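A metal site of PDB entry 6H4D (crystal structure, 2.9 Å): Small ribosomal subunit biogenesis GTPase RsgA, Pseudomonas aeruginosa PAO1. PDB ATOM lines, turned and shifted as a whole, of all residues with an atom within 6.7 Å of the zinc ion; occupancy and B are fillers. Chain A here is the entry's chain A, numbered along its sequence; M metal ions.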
ATOM      1  N   ARG A 278     -24.427   0.580  21.327  1.00  0.00           N
ATOM      2  CA  ARG A 278     -23.043   0.642  21.786  1.00  0.00           C
ATOM      3  C   ARG A 278     -22.987   0.653  23.310  1.00  0.00           C
ATOM      4  O   ARG A 278     -22.128   0.016  23.912  1.00  0.00           O
ATOM      5  CB  ARG A 278     -22.330   1.871  21.224  1.00  0.00           C
ATOM      6  CG  ARG A 278     -21.044   2.231  21.937  1.00  0.00           C
ATOM      7  CD  ARG A 278     -20.459   3.565  21.464  1.00  0.00           C
ATOM      8  NE  ARG A 278     -19.687   4.221  22.524  1.00  0.00           N
ATOM      9  CZ  ARG A 278     -19.011   5.352  22.374  1.00  0.00           C
ATOM     10  NH1 ARG A 278     -18.338   5.862  23.392  1.00  0.00           N
ATOM     11  NH2 ARG A 278     -18.997   5.973  21.196  1.00  0.00           N
ATOM     12  N   LEU A 292     -16.794   3.818  32.499  1.00  0.00           N
ATOM     13  CA  LEU A 292     -17.588   4.561  31.519  1.00  0.00           C
ATOM     14  C   LEU A 292     -18.207   5.842  32.100  1.00  0.00           C
ATOM     15  O   LEU A 292     -18.992   5.798  33.053  1.00  0.00           O
ATOM     16  CB  LEU A 292     -18.701   3.654  30.988  1.00  0.00           C
ATOM     17  CG  LEU A 292     -18.249   2.447  30.167  1.00  0.00           C
ATOM     18  CD1 LEU A 292     -19.396   1.456  29.972  1.00  0.00           C
ATOM     19  CD2 LEU A 292     -17.697   2.917  28.835  1.00  0.00           C
ATOM     20  N   CYS A 295     -14.073   9.152  30.853  1.00  0.00           N
ATOM     21  CA  CYS A 295     -13.236   9.568  29.751  1.00  0.00           C
ATOM     22  C   CYS A 295     -13.644  11.018  29.664  1.00  0.00           C
ATOM     23  O   CYS A 295     -14.833  11.300  29.681  1.00  0.00           O
ATOM     24  CB  CYS A 295     -13.638   8.878  28.445  1.00  0.00           C
ATOM     25  SG  CYS A 295     -13.344   7.111  28.317  1.00  0.00           S
ATOM     26  N   ARG A 296     -12.705  11.960  29.580  1.00  0.00           N
ATOM     27  CA  ARG A 296     -13.077  13.381  29.602  1.00  0.00           C
ATOM     28  C   ARG A 296     -14.045  13.730  28.493  1.00  0.00           C
ATOM     29  O   ARG A 296     -15.062  14.381  28.709  1.00  0.00           O
ATOM     30  CB  ARG A 296     -11.850  14.271  29.449  1.00  0.00           C
ATOM     31  CG  ARG A 296     -10.689  13.964  30.396  1.00  0.00           C
ATOM     32  CD  ARG A 296      -9.484  14.811  30.006  1.00  0.00           C
ATOM     33  NE  ARG A 296      -8.221  14.281  30.508  1.00  0.00           N
ATOM     34  CZ  ARG A 296      -7.063  14.421  29.874  1.00  0.00           C
ATOM     35  NH1 ARG A 296      -7.023  15.054  28.708  1.00  0.00           N
ATOM     36  NH2 ARG A 296      -5.953  13.909  30.379  1.00  0.00           N
ATOM     37  N   PHE A 297     -13.729  13.273  27.303  1.00  0.00           N
ATOM     38  CA  PHE A 297     -14.591  13.444  26.139  1.00  0.00           C
ATOM     39  C   PHE A 297     -15.868  12.616  26.357  1.00  0.00           C
ATOM     40  O   PHE A 297     -15.826  11.393  26.321  1.00  0.00           O
ATOM     41  CB  PHE A 297     -13.873  13.002  24.861  1.00  0.00           C
ATOM     42  CG  PHE A 297     -12.881  14.016  24.317  1.00  0.00           C
ATOM     43  CD1 PHE A 297     -12.422  15.057  25.100  1.00  0.00           C
ATOM     44  CD2 PHE A 297     -12.418  13.909  23.008  1.00  0.00           C
ATOM     45  CE1 PHE A 297     -11.509  15.975  24.586  1.00  0.00           C
ATOM     46  CE2 PHE A 297     -11.507  14.821  22.502  1.00  0.00           C
ATOM     47  CZ  PHE A 297     -11.055  15.852  23.289  1.00  0.00           C
ATOM     48  N   CYS A 300     -16.299  10.390  23.669  1.00  0.00           N
ATOM     49  CA  CYS A 300     -15.184   9.465  23.405  1.00  0.00           C
ATOM     50  C   CYS A 300     -15.628   8.159  22.758  1.00  0.00           C
ATOM     51  O   CYS A 300     -16.599   7.541  23.162  1.00  0.00           O
ATOM     52  CB  CYS A 300     -14.433   9.163  24.718  1.00  0.00           C
ATOM     53  SG  CYS A 300     -12.859   8.255  24.608  1.00  0.00           S
ATOM     54  N   LYS A 301     -14.854   7.749  21.766  1.00  0.00           N
ATOM     55  CA  LYS A 301     -15.090   6.519  21.053  1.00  0.00           C
ATOM     56  C   LYS A 301     -14.089   5.468  21.505  1.00  0.00           C
ATOM     57  O   LYS A 301     -14.078   4.345  20.996  1.00  0.00           O
ATOM     58  CB  LYS A 301     -15.007   6.745  19.553  1.00  0.00           C
ATOM     59  CG  LYS A 301     -15.996   7.765  19.047  1.00  0.00           C
ATOM     60  CD  LYS A 301     -15.838   7.998  17.567  1.00  0.00           C
ATOM     61  CE  LYS A 301     -16.710   9.145  17.082  1.00  0.00           C
ATOM     62  NZ  LYS A 301     -16.585   9.361  15.621  1.00  0.00           N
ATOM     63  N   HIS A 302     -13.253   5.823  22.470  1.00  0.00           N
ATOM     64  CA  HIS A 302     -12.264   4.884  22.979  1.00  0.00           C
ATOM     65  C   HIS A 302     -11.307   4.359  21.904  1.00  0.00           C
ATOM     66  O   HIS A 302     -10.990   3.174  21.864  1.00  0.00           O
ATOM     67  CB  HIS A 302     -12.991   3.694  23.611  1.00  0.00           C
ATOM     68  CG  HIS A 302     -14.263   4.060  24.292  1.00  0.00           C
ATOM     69  ND1 HIS A 302     -14.331   5.101  25.181  1.00  0.00           N
ATOM     70  CD2 HIS A 302     -15.509   3.551  24.214  1.00  0.00           C
ATOM     71  CE1 HIS A 302     -15.570   5.206  25.642  1.00  0.00           C
ATOM     72  NE2 HIS A 302     -16.302   4.275  25.054  1.00  0.00           N
ATOM     73  N   ASP A 303     -10.848   5.255  21.041  1.00  0.00           N
ATOM     74  CA  ASP A 303      -9.949   4.886  19.968  1.00  0.00           C
ATOM     75  C   ASP A 303      -9.006   6.033  19.619  1.00  0.00           C
ATOM     76  O   ASP A 303      -9.400   6.968  18.930  1.00  0.00           O
ATOM     77  CB  ASP A 303     -10.750   4.492  18.733  1.00  0.00           C
ATOM     78  CG  ASP A 303      -9.872   4.170  17.553  1.00  0.00           C
ATOM     79  OD1 ASP A 303      -8.642   4.141  17.717  1.00  0.00           O
ATOM     80  OD2 ASP A 303     -10.414   3.943  16.454  1.00  0.00           O
ATOM     81  N   GLU A 305      -8.072   8.199  21.422  1.00  0.00           N
ATOM     82  CA  GLU A 305      -8.494   9.397  22.099  1.00  0.00           C
ATOM     83  C   GLU A 305      -7.867   9.529  23.481  1.00  0.00           C
ATOM     84  O   GLU A 305      -8.066   8.683  24.345  1.00  0.00           O
ATOM     85  CB  GLU A 305     -10.019   9.432  22.203  1.00  0.00           C
ATOM     86  CG  GLU A 305     -10.719   9.274  20.862  1.00  0.00           C
ATOM     87  CD  GLU A 305     -12.190   8.900  20.992  1.00  0.00           C
ATOM     88  OE1 GLU A 305     -12.607   8.491  22.090  1.00  0.00           O
ATOM     89  OE2 GLU A 305     -12.904   9.004  19.984  1.00  0.00           O
ATOM     90  N   GLY A 307      -7.351  10.820  27.228  1.00  0.00           N
ATOM     91  CA  GLY A 307      -8.359  11.053  28.240  1.00  0.00           C
ATOM     92  C   GLY A 307      -9.375   9.922  28.247  1.00  0.00           C
ATOM     93  O   GLY A 307     -10.376  10.010  28.951  1.00  0.00           O
ATOM     94  N   CYS A 308      -9.114   8.870  27.474  1.00  0.00           N
ATOM     95  CA  CYS A 308     -10.022   7.717  27.417  1.00  0.00           C
ATOM     96  C   CYS A 308      -9.653   6.904  28.637  1.00  0.00           C
ATOM     97  O   CYS A 308      -8.536   6.440  28.765  1.00  0.00           O
ATOM     98  CB  CYS A 308      -9.777   6.918  26.128  1.00  0.00           C
ATOM     99  SG  CYS A 308     -10.617   5.333  25.894  1.00  0.00           S
ATOM    100  N   ALA A 309     -10.596   6.755  29.551  1.00  0.00           N
ATOM    101  CA  ALA A 309     -10.365   6.014  30.775  1.00  0.00           C
ATOM    102  C   ALA A 309     -10.066   4.566  30.480  1.00  0.00           C
ATOM    103  O   ALA A 309      -9.263   3.916  31.146  1.00  0.00           O
ATOM    104  CB  ALA A 309     -11.556   6.144  31.696  1.00  0.00           C
ATOM    105  N   LEU A 310     -10.732   4.045  29.468  1.00  0.00           N
ATOM    106  CA  LEU A 310     -10.545   2.669  29.086  1.00  0.00           C
ATOM    107  C   LEU A 310      -9.121   2.447  28.638  1.00  0.00           C
ATOM    108  O   LEU A 310      -8.510   1.450  28.984  1.00  0.00           O
ATOM    109  CB  LEU A 310     -11.515   2.300  27.964  1.00  0.00           C
ATOM    110  CG  LEU A 310     -13.000   2.501  28.254  1.00  0.00           C
ATOM    111  CD1 LEU A 310     -13.832   1.750  27.242  1.00  0.00           C
ATOM    112  CD2 LEU A 310     -13.335   2.052  29.656  1.00  0.00           C
ATOM    113  N   LEU A 311      -8.587   3.388  27.868  1.00  0.00           N
ATOM    114  CA  LEU A 311      -7.232   3.263  27.370  1.00  0.00           C
ATOM    115  C   LEU A 311      -6.224   3.249  28.485  1.00  0.00           C
ATOM    116  O   LEU A 311      -5.294   2.461  28.476  1.00  0.00           O
ATOM    117  CB  LEU A 311      -6.928   4.434  26.446  1.00  0.00           C
ATOM    118  CG  LEU A 311      -7.814   4.510  25.228  1.00  0.00           C
ATOM    119  CD1 LEU A 311      -7.297   5.555  24.256  1.00  0.00           C
ATOM    120  CD2 LEU A 311      -7.841   3.148  24.558  1.00  0.00           C
HETATM  121 ZN    ZN M   1     -12.862   6.337  26.070  1.00  0.00          ZN
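The backbone NH (N) of His 302 lies within hydrogen-bond range of the side-chain carboxylate (OE1) of Glu 305 (2.8 Å). The guanidinium group of Arg 278 sits at hydrogen-bond distance from a ring nitrogen (NE2) of His 302 (3.1 Å). The side-chain carboxylate (OE1) of Glu 305 lies close to the side-chain sulfur (SG) of Cys 300. The backbone carbonyl oxygen (O) of Cys 300 is in hydrogen-bond range of the guanidinium group (NH1) of Arg 278. The side-chain sulfur of Cys 295 sits close to the backbone NH of Ala 309 (3.0 Å). SG of Cys 308 lies close to N of Leu 311 (3.4 Å).
Of the 15 residues printed, 4 come within 4 Å of the zinc ion. The nearest printed residue that does not touch the zinc ion is Ala 309 (4.2 Å).
The zinc ion is bound by ND1 of His 302, SG of Cys 300, SG of Cys 295 and SG of Cys 308. The zinc ion has four donor atoms within binding distance.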
